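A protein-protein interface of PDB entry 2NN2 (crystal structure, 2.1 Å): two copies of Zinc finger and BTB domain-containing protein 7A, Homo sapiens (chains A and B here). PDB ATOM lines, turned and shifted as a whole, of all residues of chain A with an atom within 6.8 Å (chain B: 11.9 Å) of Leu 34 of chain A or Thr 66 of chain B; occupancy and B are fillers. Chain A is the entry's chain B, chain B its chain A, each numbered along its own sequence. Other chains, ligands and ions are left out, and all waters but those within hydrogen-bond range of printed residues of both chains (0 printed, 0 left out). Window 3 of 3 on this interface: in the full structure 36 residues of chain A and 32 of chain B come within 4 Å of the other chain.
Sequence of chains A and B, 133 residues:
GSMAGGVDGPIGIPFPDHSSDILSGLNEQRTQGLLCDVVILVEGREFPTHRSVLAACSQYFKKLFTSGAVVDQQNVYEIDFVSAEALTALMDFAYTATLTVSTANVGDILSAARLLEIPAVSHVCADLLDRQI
O of Ser 52 of chain B sits at hydrogen-bond distance from NE2 of Gln 29 of chain A (3.1 Å).
The backbone carbonyl oxygen (O) of Lys 62 of chain B sits at hydrogen-bond distance from the side-chain hydroxyl (OG1) of Thr 66 of chain B, 2.7 Å away. The backbone carbonyl oxygen (O) of Gln 29 of chain A lies within hydrogen-bond range of the backbone NH (N) of Leu 34 of chain A (2.8 Å). The side-chain amide oxygen of Gln 29 of chain A sits at hydrogen-bond distance from a ring nitrogen (NE2) of His 50 of chain A (2.9 Å). The backbone carbonyl oxygen of Leu 34 of chain A lies within hydrogen-bond range of the side-chain sulfur of Cys 36 of chain A (3.6 Å).
Among the printed residues, pairs that only touch across the chains: Leu 35 of chain A with Phe 65 of chain B (3.4 Å), His 50 of chain A with Ser 52 of chain B (3.6 Å), Leu 35 of chain A with Ala 55 of chain B (3.6 Å), Leu 26 of chain A with Ser 52 of chain B (3.8 Å), Leu 34 of chain A with Thr 66 of chain B (3.8 Å), Gln 29 of chain A with Ala 55 of chain B (3.9 Å) and Gln 29 of chain A with Ala 56 of chain B (3.95 Å).
Printed residues of chain B within 4 Å of Leu 26 of chain A: Ser 52 (3.8 Å). Arg 30 of chain A touches none of the printed residues of chain B. No residue of chain B comes within 4 Å of Gly 33 of chain A. Of the printed residues of chain B, Leu 34 of chain A touches Thr 66 (3.8 Å). Leu 35 of chain A touches just these residues of chain B: Ala 55 (3.6 Å) and Phe 65 (3.4 Å). No residue of chain B comes within 4 Å of Cys 36 of chain A. Of the printed residues of chain B, His 50 of chain A touches Ser 52 (3.6 Å). Of the printed residues of chain A, Ser 52 of chain B touches Leu 26, Gln 29 and His 50. Leu 54 of chain B touches none of the printed residues of chain A. Of the printed residues of chain A, Ala 56 of chain B touches Gln 29 (3.95 Å). Of the printed residues of chain A, Phe 65 of chain B touches Leu 35. Of chain A, only Leu 34 comes within 4 Å of Thr 66 of chain B. The nearest residue of chain B that does not touch Leu 34 of chain A is Lys 62 of chain B (5.5 Å).
Printed residues of chain A that touch a printed residue of chain B: Leu 26, Gln 29, Leu 34, Leu 35 and His 50. Hydrophobic or aromatic side chains of chain A within 4 Å of the printed part of chain B: Leu 26, Leu 34, Leu 35 and His 50. Hydrophobic or aromatic side chains of chain B that line the printed part of chain A: Ala 55 and Phe 65. Along chain B the printed residues that touch a printed residue of chain A span positions 52 to 66. Among the printed residues, 8 pairs touch across the chains.
2 positions are printed for both chains.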
ATOM      1  N   LEU A  26     -11.050 -16.741  31.681  1.00  0.00           N
ATOM      2  CA  LEU A  26      -9.622 -17.001  31.571  1.00  0.00           C
ATOM      3  C   LEU A  26      -9.340 -18.495  31.777  1.00  0.00           C
ATOM      4  O   LEU A  26      -8.507 -19.091  31.066  1.00  0.00           O
ATOM      5  CB  LEU A  26      -8.805 -16.081  32.535  1.00  0.00           C
ATOM      6  CG  LEU A  26      -8.898 -14.581  32.258  1.00  0.00           C
ATOM      7  CD1 LEU A  26      -8.171 -13.677  33.328  1.00  0.00           C
ATOM      8  CD2 LEU A  26      -8.301 -14.319  30.916  1.00  0.00           C
ATOM      9  N   GLU A  28     -11.439 -21.049  31.215  1.00  0.00           N
ATOM     10  CA  GLU A  28     -11.910 -21.739  29.990  1.00  0.00           C
ATOM     11  C   GLU A  28     -10.860 -21.624  28.876  1.00  0.00           C
ATOM     12  O   GLU A  28     -10.617 -22.578  28.144  1.00  0.00           O
ATOM     13  CB  GLU A  28     -13.248 -21.150  29.485  1.00  0.00           C
ATOM     14  CG  GLU A  28     -14.488 -21.514  30.326  1.00  0.00           C
ATOM     15  CD  GLU A  28     -15.830 -21.346  29.567  1.00  0.00           C
ATOM     16  OE1 GLU A  28     -15.866 -21.467  28.298  1.00  0.00           O
ATOM     17  OE2 GLU A  28     -16.873 -21.097  30.248  1.00  0.00           O
ATOM     18  N   GLN A  29     -10.254 -20.445  28.734  1.00  0.00           N
ATOM     19  CA  GLN A  29      -9.188 -20.256  27.743  1.00  0.00           C
ATOM     20  C   GLN A  29      -8.022 -21.195  27.958  1.00  0.00           C
ATOM     21  O   GLN A  29      -7.574 -21.841  27.012  1.00  0.00           O
ATOM     22  CB  GLN A  29      -8.681 -18.823  27.725  1.00  0.00           C
ATOM     23  CG  GLN A  29      -9.590 -17.878  26.917  1.00  0.00           C
ATOM     24  CD  GLN A  29      -9.268 -16.452  27.249  1.00  0.00           C
ATOM     25  OE1 GLN A  29      -8.119 -16.136  27.578  1.00  0.00           O
ATOM     26  NE2 GLN A  29     -10.268 -15.572  27.185  1.00  0.00           N
ATOM     27  N   ARG A  30      -7.548 -21.252  29.202  1.00  0.00           N
ATOM     28  CA  ARG A  30      -6.445 -22.100  29.607  1.00  0.00           C
ATOM     29  C   ARG A  30      -6.740 -23.576  29.446  1.00  0.00           C
ATOM     30  O   ARG A  30      -5.854 -24.337  29.070  1.00  0.00           O
ATOM     31  CB  ARG A  30      -6.086 -21.857  31.084  1.00  0.00           C
ATOM     32  CG  ARG A  30      -5.448 -23.055  31.678  1.00  0.00           C
ATOM     33  CD  ARG A  30      -5.251 -23.057  33.143  1.00  0.00           C
ATOM     34  NE  ARG A  30      -6.412 -23.422  33.952  1.00  0.00           N
ATOM     35  CZ  ARG A  30      -6.326 -24.228  35.001  1.00  0.00           C
ATOM     36  NH1 ARG A  30      -5.157 -24.785  35.294  1.00  0.00           N
ATOM     37  NH2 ARG A  30      -7.365 -24.469  35.758  1.00  0.00           N
ATOM     38  N   THR A  31      -7.945 -23.982  29.824  1.00  0.00           N
ATOM     39  CA  THR A  31      -8.358 -25.386  29.824  1.00  0.00           C
ATOM     40  C   THR A  31      -8.354 -25.914  28.400  1.00  0.00           C
ATOM     41  O   THR A  31      -7.993 -27.060  28.170  1.00  0.00           O
ATOM     42  CB  THR A  31      -9.736 -25.556  30.506  1.00  0.00           C
ATOM     43  OG1 THR A  31      -9.600 -25.302  31.917  1.00  0.00           O
ATOM     44  CG2 THR A  31     -10.268 -26.952  30.315  1.00  0.00           C
ATOM     45  N   GLN A  32      -8.711 -25.056  27.458  1.00  0.00           N
ATOM     46  CA  GLN A  32      -8.716 -25.360  26.036  1.00  0.00           C
ATOM     47  C   GLN A  32      -7.470 -25.018  25.222  1.00  0.00           C
ATOM     48  O   GLN A  32      -7.408 -25.378  24.061  1.00  0.00           O
ATOM     49  CB  GLN A  32      -9.914 -24.678  25.387  1.00  0.00           C
ATOM     50  CG  GLN A  32     -11.199 -25.461  25.641  1.00  0.00           C
ATOM     51  CD  GLN A  32     -12.432 -24.601  25.675  1.00  0.00           C
ATOM     52  OE1 GLN A  32     -12.440 -23.457  25.169  1.00  0.00           O
ATOM     53  NE2 GLN A  32     -13.508 -25.144  26.278  1.00  0.00           N
ATOM     54  N   GLY A  33      -6.489 -24.313  25.794  1.00  0.00           N
ATOM     55  CA  GLY A  33      -5.311 -23.888  25.012  1.00  0.00           C
ATOM     56  C   GLY A  33      -5.600 -22.746  24.037  1.00  0.00           C
ATOM     57  O   GLY A  33      -4.970 -22.622  22.974  1.00  0.00           O
ATOM     58  N   LEU A  34      -6.542 -21.888  24.401  1.00  0.00           N
ATOM     59  CA  LEU A  34      -6.967 -20.824  23.520  1.00  0.00           C
ATOM     60  C   LEU A  34      -6.449 -19.476  24.037  1.00  0.00           C
ATOM     61  O   LEU A  34      -6.509 -19.217  25.238  1.00  0.00           O
ATOM     62  CB  LEU A  34      -8.481 -20.838  23.495  1.00  0.00           C
ATOM     63  CG  LEU A  34      -9.259 -20.123  22.402  1.00  0.00           C
ATOM     64  CD1 LEU A  34      -8.801 -20.538  20.980  1.00  0.00           C
ATOM     65  CD2 LEU A  34     -10.753 -20.431  22.640  1.00  0.00           C
ATOM     66  N   LEU A  35      -5.947 -18.624  23.150  1.00  0.00           N
ATOM     67  CA  LEU A  35      -5.378 -17.301  23.538  1.00  0.00           C
ATOM     68  C   LEU A  35      -4.312 -17.306  24.642  1.00  0.00           C
ATOM     69  O   LEU A  35      -4.091 -16.301  25.323  1.00  0.00           O
ATOM     70  CB  LEU A  35      -6.487 -16.302  23.895  1.00  0.00           C
ATOM     71  CG  LEU A  35      -7.489 -16.012  22.769  1.00  0.00           C
ATOM     72  CD1 LEU A  35      -8.441 -14.965  23.213  1.00  0.00           C
ATOM     73  CD2 LEU A  35      -6.778 -15.569  21.458  1.00  0.00           C
ATOM     74  N   CYS A  36      -3.660 -18.450  24.805  1.00  0.00           N
ATOM     75  CA  CYS A  36      -2.580 -18.641  25.770  1.00  0.00           C
ATOM     76  C   CYS A  36      -1.263 -18.237  25.114  1.00  0.00           C
ATOM     77  O   CYS A  36      -0.966 -18.650  23.986  1.00  0.00           O
ATOM     78  CB  CYS A  36      -2.546 -20.105  26.192  1.00  0.00           C
ATOM     79  SG  CYS A  36      -3.886 -20.541  27.331  1.00  0.00           S
ATOM     80  N   ASP A  37      -0.470 -17.427  25.807  1.00  0.00           N
ATOM     81  CA  ASP A  37       0.715 -16.857  25.181  1.00  0.00           C
ATOM     82  C   ASP A  37       2.047 -17.472  25.651  1.00  0.00           C
ATOM     83  O   ASP A  37       3.094 -17.090  25.160  1.00  0.00           O
ATOM     84  CB  ASP A  37       0.728 -15.360  25.436  1.00  0.00           C
ATOM     85  CG  ASP A  37       0.508 -15.023  26.916  1.00  0.00           C
ATOM     86  OD1 ASP A  37       1.485 -15.026  27.681  1.00  0.00           O
ATOM     87  OD2 ASP A  37      -0.643 -14.739  27.312  1.00  0.00           O
ATOM     88  N   PRO A  48      -0.330 -24.809  29.185  1.00  0.00           N
ATOM     89  CA  PRO A  48      -0.560 -23.531  28.469  1.00  0.00           C
ATOM     90  C   PRO A  48      -1.218 -22.476  29.371  1.00  0.00           C
ATOM     91  O   PRO A  48      -2.205 -22.762  30.031  1.00  0.00           O
ATOM     92  CB  PRO A  48      -1.489 -23.933  27.334  1.00  0.00           C
ATOM     93  CG  PRO A  48      -1.307 -25.492  27.244  1.00  0.00           C
ATOM     94  CD  PRO A  48      -1.167 -25.894  28.640  1.00  0.00           C
ATOM     95  N   HIS A  50      -1.326 -17.865  30.678  1.00  0.00           N
ATOM     96  CA  HIS A  50      -1.218 -16.464  30.316  1.00  0.00           C
ATOM     97  C   HIS A  50      -0.194 -15.815  31.235  1.00  0.00           C
ATOM     98  O   HIS A  50      -0.352 -15.854  32.439  1.00  0.00           O
ATOM     99  CB  HIS A  50      -2.534 -15.698  30.583  1.00  0.00           C
ATOM    100  CG  HIS A  50      -3.757 -16.310  29.972  1.00  0.00           C
ATOM    101  ND1 HIS A  50      -4.508 -17.267  30.617  1.00  0.00           N
ATOM    102  CD2 HIS A  50      -4.400 -16.042  28.815  1.00  0.00           C
ATOM    103  CE1 HIS A  50      -5.557 -17.577  29.865  1.00  0.00           C
ATOM    104  NE2 HIS A  50      -5.516 -16.837  28.770  1.00  0.00           N
ATOM    105  N   ASP B  37      -0.743  -7.122  25.318  1.00  0.00           N
ATOM    106  CA  ASP B  37      -0.363  -7.733  24.055  1.00  0.00           C
ATOM    107  C   ASP B  37      -1.118  -7.125  22.888  1.00  0.00           C
ATOM    108  O   ASP B  37      -0.958  -7.549  21.750  1.00  0.00           O
ATOM    109  CB  ASP B  37      -0.653  -9.226  24.113  1.00  0.00           C
ATOM    110  CG  ASP B  37      -2.058  -9.529  24.677  1.00  0.00           C
ATOM    111  OD1 ASP B  37      -3.026  -9.528  23.890  1.00  0.00           O
ATOM    112  OD2 ASP B  37      -2.175  -9.767  25.907  1.00  0.00           O
ATOM    113  N   VAL B  38      -1.954  -6.128  23.163  1.00  0.00           N
ATOM    114  CA  VAL B  38      -2.743  -5.540  22.078  1.00  0.00           C
ATOM    115  C   VAL B  38      -3.043  -4.088  22.442  1.00  0.00           C
ATOM    116  O   VAL B  38      -3.017  -3.699  23.638  1.00  0.00           O
ATOM    117  CB  VAL B  38      -4.017  -6.429  21.718  1.00  0.00           C
ATOM    118  CG1 VAL B  38      -5.120  -6.290  22.755  1.00  0.00           C
ATOM    119  CG2 VAL B  38      -4.556  -6.125  20.334  1.00  0.00           C
ATOM    120  N   HIS B  50      -5.267  -6.629  27.035  1.00  0.00           N
ATOM    121  CA  HIS B  50      -4.936  -8.033  26.910  1.00  0.00           C
ATOM    122  C   HIS B  50      -5.998  -8.650  26.025  1.00  0.00           C
ATOM    123  O   HIS B  50      -7.196  -8.537  26.317  1.00  0.00           O
ATOM    124  CB  HIS B  50      -4.941  -8.720  28.311  1.00  0.00           C
ATOM    125  CG  HIS B  50      -4.074  -8.056  29.338  1.00  0.00           C
ATOM    126  ND1 HIS B  50      -4.540  -7.069  30.177  1.00  0.00           N
ATOM    127  CD2 HIS B  50      -2.800  -8.306  29.732  1.00  0.00           C
ATOM    128  CE1 HIS B  50      -3.576  -6.681  30.991  1.00  0.00           C
ATOM    129  NE2 HIS B  50      -2.512  -7.429  30.753  1.00  0.00           N
ATOM    130  N   ARG B  51      -5.614  -9.347  24.973  1.00  0.00           N
ATOM    131  CA  ARG B  51      -6.628 -10.009  24.193  1.00  0.00           C
ATOM    132  C   ARG B  51      -7.459 -11.026  25.020  1.00  0.00           C
ATOM    133  O   ARG B  51      -8.661 -11.172  24.821  1.00  0.00           O
ATOM    134  CB  ARG B  51      -6.074 -10.590  22.873  1.00  0.00           C
ATOM    135  CG  ARG B  51      -4.980 -11.639  22.981  1.00  0.00           C
ATOM    136  CD  ARG B  51      -4.327 -11.834  21.569  1.00  0.00           C
ATOM    137  NE  ARG B  51      -3.396 -10.763  21.253  1.00  0.00           N
ATOM    138  CZ  ARG B  51      -3.206 -10.258  20.038  1.00  0.00           C
ATOM    139  NH1 ARG B  51      -3.888 -10.737  19.000  1.00  0.00           N
ATOM    140  NH2 ARG B  51      -2.338  -9.263  19.869  1.00  0.00           N
ATOM    141  N   SER B  52      -6.834 -11.659  26.009  1.00  0.00           N
ATOM    142  CA  SER B  52      -7.512 -12.662  26.840  1.00  0.00           C
ATOM    143  C   SER B  52      -8.659 -12.053  27.652  1.00  0.00           C
ATOM    144  O   SER B  52      -9.742 -12.606  27.729  1.00  0.00           O
ATOM    145  CB  SER B  52      -6.471 -13.361  27.742  1.00  0.00           C
ATOM    146  OG  SER B  52      -5.873 -12.405  28.649  1.00  0.00           O
ATOM    147  N   VAL B  53      -8.394 -10.945  28.306  1.00  0.00           N
ATOM    148  CA  VAL B  53      -9.412 -10.254  29.092  1.00  0.00           C
ATOM    149  C   VAL B  53     -10.553  -9.717  28.205  1.00  0.00           C
ATOM    150  O   VAL B  53     -11.739  -9.812  28.577  1.00  0.00           O
ATOM    151  CB  VAL B  53      -8.803  -9.075  29.879  1.00  0.00           C
ATOM    152  CG1 VAL B  53      -9.926  -8.250  30.565  1.00  0.00           C
ATOM    153  CG2 VAL B  53      -7.793  -9.549  30.887  1.00  0.00           C
ATOM    154  N   LEU B  54     -10.214  -9.141  27.044  1.00  0.00           N
ATOM    155  CA  LEU B  54     -11.250  -8.676  26.087  1.00  0.00           C
ATOM    156  C   LEU B  54     -12.138  -9.819  25.650  1.00  0.00           C
ATOM    157  O   LEU B  54     -13.360  -9.679  25.640  1.00  0.00           O
ATOM    158  CB  LEU B  54     -10.618  -8.028  24.843  1.00  0.00           C
ATOM    159  CG  LEU B  54      -9.730  -6.784  25.017  1.00  0.00           C
ATOM    160  CD1 LEU B  54      -9.275  -6.186  23.654  1.00  0.00           C
ATOM    161  CD2 LEU B  54     -10.485  -5.752  25.839  1.00  0.00           C
ATOM    162  N   ALA B  55     -11.543 -10.966  25.333  1.00  0.00           N
ATOM    163  CA  ALA B  55     -12.319 -12.137  24.875  1.00  0.00           C
ATOM    164  C   ALA B  55     -13.196 -12.739  25.977  1.00  0.00           C
ATOM    165  O   ALA B  55     -14.197 -13.393  25.682  1.00  0.00           O
ATOM    166  CB  ALA B  55     -11.389 -13.220  24.332  1.00  0.00           C
ATOM    167  N   ALA B  56     -12.812 -12.548  27.232  1.00  0.00           N
ATOM    168  CA  ALA B  56     -13.577 -13.147  28.379  1.00  0.00           C
ATOM    169  C   ALA B  56     -14.853 -12.302  28.649  1.00  0.00           C
ATOM    170  O   ALA B  56     -15.779 -12.723  29.370  1.00  0.00           O
ATOM    171  CB  ALA B  56     -12.710 -13.222  29.610  1.00  0.00           C
ATOM    172  N   CYS B  57     -14.895 -11.131  28.016  1.00  0.00           N
ATOM    173  CA  CYS B  57     -15.849 -10.067  28.306  1.00  0.00           C
ATOM    174  C   CYS B  57     -16.797  -9.742  27.136  1.00  0.00           C
ATOM    175  O   CYS B  57     -17.940  -9.306  27.335  1.00  0.00           O
ATOM    176  CB  CYS B  57     -14.983  -8.833  28.536  1.00  0.00           C
ATOM    177  SG  CYS B  57     -15.655  -7.598  29.521  1.00  0.00           S
ATOM    178  N   SER B  58     -16.284  -9.902  25.915  1.00  0.00           N
ATOM    179  CA  SER B  58     -16.879  -9.383  24.714  1.00  0.00           C
ATOM    180  C   SER B  58     -16.819 -10.501  23.691  1.00  0.00           C
ATOM    181  O   SER B  58     -15.723 -10.990  23.367  1.00  0.00           O
ATOM    182  CB  SER B  58     -16.046  -8.186  24.246  1.00  0.00           C
ATOM    183  OG  SER B  58     -16.195  -7.928  22.859  1.00  0.00           O
ATOM    184  N   GLN B  59     -17.984 -10.914  23.193  1.00  0.00           N
ATOM    185  CA  GLN B  59     -18.068 -11.938  22.147  1.00  0.00           C
ATOM    186  C   GLN B  59     -17.512 -11.476  20.776  1.00  0.00           C
ATOM    187  O   GLN B  59     -17.039 -12.301  19.999  1.00  0.00           O
ATOM    188  CB  GLN B  59     -19.495 -12.487  22.017  1.00  0.00           C
ATOM    189  CG  GLN B  59     -19.586 -13.678  21.063  1.00  0.00           C
ATOM    190  CD  GLN B  59     -18.997 -14.963  21.660  1.00  0.00           C
ATOM    191  OE1 GLN B  59     -18.882 -15.099  22.881  1.00  0.00           O
ATOM    192  NE2 GLN B  59     -18.624 -15.913  20.789  1.00  0.00           N
ATOM    193  N   TYR B  60     -17.562 -10.169  20.515  1.00  0.00           N
ATOM    194  CA  TYR B  60     -16.946  -9.547  19.355  1.00  0.00           C
ATOM    195  C   TYR B  60     -15.427  -9.721  19.354  1.00  0.00           C
ATOM    196  O   TYR B  60     -14.855 -10.118  18.352  1.00  0.00           O
ATOM    197  CB  TYR B  60     -17.241  -8.049  19.309  1.00  0.00           C
ATOM    198  CG  TYR B  60     -16.516  -7.394  18.159  1.00  0.00           C
ATOM    199  CD1 TYR B  60     -17.014  -7.487  16.862  1.00  0.00           C
ATOM    200  CD2 TYR B  60     -15.295  -6.745  18.360  1.00  0.00           C
ATOM    201  CE1 TYR B  60     -16.308  -6.918  15.776  1.00  0.00           C
ATOM    202  CE2 TYR B  60     -14.587  -6.186  17.304  1.00  0.00           C
ATOM    203  CZ  TYR B  60     -15.107  -6.285  16.014  1.00  0.00           C
ATOM    204  OH  TYR B  60     -14.415  -5.718  14.979  1.00  0.00           O
ATOM    205  N   PHE B  61     -14.778  -9.355  20.466  1.00  0.00           N
ATOM    206  CA  PHE B  61     -13.333  -9.527  20.608  1.00  0.00           C
ATOM    207  C   PHE B  61     -12.899 -10.987  20.686  1.00  0.00           C
ATOM    208  O   PHE B  61     -11.808 -11.344  20.219  1.00  0.00           O
ATOM    209  CB  PHE B  61     -12.807  -8.749  21.807  1.00  0.00           C
ATOM    210  CG  PHE B  61     -12.696  -7.271  21.582  1.00  0.00           C
ATOM    211  CD1 PHE B  61     -11.945  -6.758  20.513  1.00  0.00           C
ATOM    212  CD2 PHE B  61     -13.346  -6.376  22.432  1.00  0.00           C
ATOM    213  CE1 PHE B  61     -11.833  -5.377  20.314  1.00  0.00           C
ATOM    214  CE2 PHE B  61     -13.205  -5.013  22.266  1.00  0.00           C
ATOM    215  CZ  PHE B  61     -12.477  -4.509  21.185  1.00  0.00           C
ATOM    216  N   LYS B  62     -13.740 -11.845  21.253  1.00  0.00           N
ATOM    217  CA  LYS B  62     -13.435 -13.281  21.287  1.00  0.00           C
ATOM    218  C   LYS B  62     -13.379 -13.885  19.877  1.00  0.00           C
ATOM    219  O   LYS B  62     -12.491 -14.685  19.563  1.00  0.00           O
ATOM    220  CB  LYS B  62     -14.462 -14.026  22.135  1.00  0.00           C
ATOM    221  CG  LYS B  62     -14.359 -15.544  22.107  1.00  0.00           C
ATOM    222  CD  LYS B  62     -14.994 -16.119  23.383  1.00  0.00           C
ATOM    223  CE  LYS B  62     -15.391 -17.602  23.282  1.00  0.00           C
ATOM    224  NZ  LYS B  62     -16.517 -17.893  24.255  1.00  0.00           N
ATOM    225  N   LYS B  63     -14.361 -13.507  19.057  1.00  0.00           N
ATOM    226  CA  LYS B  63     -14.422 -13.846  17.641  1.00  0.00           C
ATOM    227  C   LYS B  63     -13.235 -13.260  16.857  1.00  0.00           C
ATOM    228  O   LYS B  63     -12.565 -13.979  16.105  1.00  0.00           O
ATOM    229  CB  LYS B  63     -15.730 -13.312  17.071  1.00  0.00           C
ATOM    230  CG  LYS B  63     -16.339 -14.117  15.919  1.00  0.00           C
ATOM    231  CD  LYS B  63     -17.863 -13.782  15.737  1.00  0.00           C
ATOM    232  CE  LYS B  63     -18.624 -13.588  17.073  1.00  0.00           C
ATOM    233  NZ  LYS B  63     -19.889 -14.432  17.192  1.00  0.00           N
ATOM    234  N   LEU B  64     -12.978 -11.967  17.030  1.00  0.00           N
ATOM    235  CA  LEU B  64     -11.818 -11.309  16.401  1.00  0.00           C
ATOM    236  C   LEU B  64     -10.450 -11.972  16.707  1.00  0.00           C
ATOM    237  O   LEU B  64      -9.603 -12.102  15.816  1.00  0.00           O
ATOM    238  CB  LEU B  64     -11.780  -9.813  16.748  1.00  0.00           C
ATOM    239  CG  LEU B  64     -10.686  -8.834  16.275  1.00  0.00           C
ATOM    240  CD1 LEU B  64     -10.786  -8.493  14.807  1.00  0.00           C
ATOM    241  CD2 LEU B  64     -10.748  -7.555  17.063  1.00  0.00           C
ATOM    242  N   PHE B  65     -10.220 -12.367  17.955  1.00  0.00           N
ATOM    243  CA  PHE B  65      -8.898 -12.863  18.345  1.00  0.00           C
ATOM    244  C   PHE B  65      -8.672 -14.369  18.144  1.00  0.00           C
ATOM    245  O   PHE B  65      -7.551 -14.860  18.276  1.00  0.00           O
ATOM    246  CB  PHE B  65      -8.560 -12.447  19.778  1.00  0.00           C
ATOM    247  CG  PHE B  65      -8.466 -10.957  19.971  1.00  0.00           C
ATOM    248  CD1 PHE B  65      -7.777 -10.167  19.074  1.00  0.00           C
ATOM    249  CD2 PHE B  65      -9.067 -10.343  21.070  1.00  0.00           C
ATOM    250  CE1 PHE B  65      -7.692  -8.779  19.256  1.00  0.00           C
ATOM    251  CE2 PHE B  65      -8.974  -8.969  21.266  1.00  0.00           C
ATOM    252  CZ  PHE B  65      -8.309  -8.188  20.347  1.00  0.00           C
ATOM    253  N   THR B  66      -9.727 -15.105  17.831  1.00  0.00           N
ATOM    254  CA  THR B  66      -9.604 -16.562  17.589  1.00  0.00           C
ATOM    255  C   THR B  66      -9.869 -16.893  16.115  1.00  0.00           C
ATOM    256  O   THR B  66      -9.985 -18.072  15.732  1.00  0.00           O
ATOM    257  CB  THR B  66     -10.560 -17.360  18.467  1.00  0.00           C
ATOM    258  OG1 THR B  66     -11.900 -16.929  18.209  1.00  0.00           O
ATOM    259  CG2 THR B  66     -10.232 -17.168  19.938  1.00  0.00           C
ATOM    260  N   SER B  67      -9.959 -15.824  15.315  1.00  0.00           N
ATOM    261  CA  SER B  67     -10.154 -15.853  13.858  1.00  0.00           C
ATOM    262  C   SER B  67     -11.478 -16.473  13.417  1.00  0.00           C
ATOM    263  O   SER B  67     -12.498 -15.771  13.358  1.00  0.00           O
ATOM    264  CB  SER B  67      -8.952 -16.493  13.144  1.00  0.00           C
ATOM    265  OG  SER B  67      -7.841 -15.610  13.184  1.00  0.00           O
ATOM    266  N   GLN B  74      -1.639  -8.807  14.285  1.00  0.00           N
ATOM    267  CA  GLN B  74      -1.533  -7.389  14.616  1.00  0.00           C
ATOM    268  C   GLN B  74      -1.266  -7.168  16.117  1.00  0.00           C
ATOM    269  O   GLN B  74      -1.680  -7.965  16.964  1.00  0.00           O
ATOM    270  CB  GLN B  74      -2.801  -6.615  14.155  1.00  0.00           C
ATOM    271  CG  GLN B  74      -3.082  -6.668  12.639  1.00  0.00           C
ATOM    272  CD  GLN B  74      -4.529  -6.303  12.239  1.00  0.00           C
ATOM    273  OE1 GLN B  74      -5.029  -5.207  12.539  1.00  0.00           O
ATOM    274  NE2 GLN B  74      -5.197  -7.228  11.529  1.00  0.00           N
ATOM    275  N   TYR B  77      -5.283  -2.601  16.722  1.00  0.00           N
ATOM    276  CA  TYR B  77      -6.590  -2.774  16.095  1.00  0.00           C
ATOM    277  C   TYR B  77      -7.365  -1.473  16.174  1.00  0.00           C
ATOM    278  O   TYR B  77      -7.536  -0.923  17.251  1.00  0.00           O
ATOM    279  CB  TYR B  77      -7.368  -3.909  16.780  1.00  0.00           C
ATOM    280  CG  TYR B  77      -6.828  -5.286  16.494  1.00  0.00           C
ATOM    281  CD1 TYR B  77      -5.773  -5.821  17.227  1.00  0.00           C
ATOM    282  CD2 TYR B  77      -7.382  -6.052  15.492  1.00  0.00           C
ATOM    283  CE1 TYR B  77      -5.290  -7.099  16.966  1.00  0.00           C
ATOM    284  CE2 TYR B  77      -6.918  -7.322  15.221  1.00  0.00           C
ATOM    285  CZ  TYR B  77      -5.882  -7.836  15.951  1.00  0.00           C
ATOM    286  OH  TYR B  77      -5.473  -9.094  15.644  1.00  0.00           O
ATOM    287  N   GLU B 117     -20.879  -6.724  22.112  1.00  0.00           N
ATOM    288  CA  GLU B 117     -21.510  -7.940  22.651  1.00  0.00           C
ATOM    289  C   GLU B 117     -21.009  -8.228  24.071  1.00  0.00           C
ATOM    290  O   GLU B 117     -20.488  -9.328  24.370  1.00  0.00           O
ATOM    291  CB  GLU B 117     -21.362  -9.158  21.719  1.00  0.00           C
ATOM    292  CG  GLU B 117     -21.825  -8.943  20.258  1.00  0.00           C
ATOM    293  CD  GLU B 117     -21.659 -10.188  19.366  1.00  0.00           C
ATOM    294  OE1 GLU B 117     -22.443 -11.164  19.524  1.00  0.00           O
ATOM    295  OE2 GLU B 117     -20.749 -10.191  18.490  1.00  0.00           O
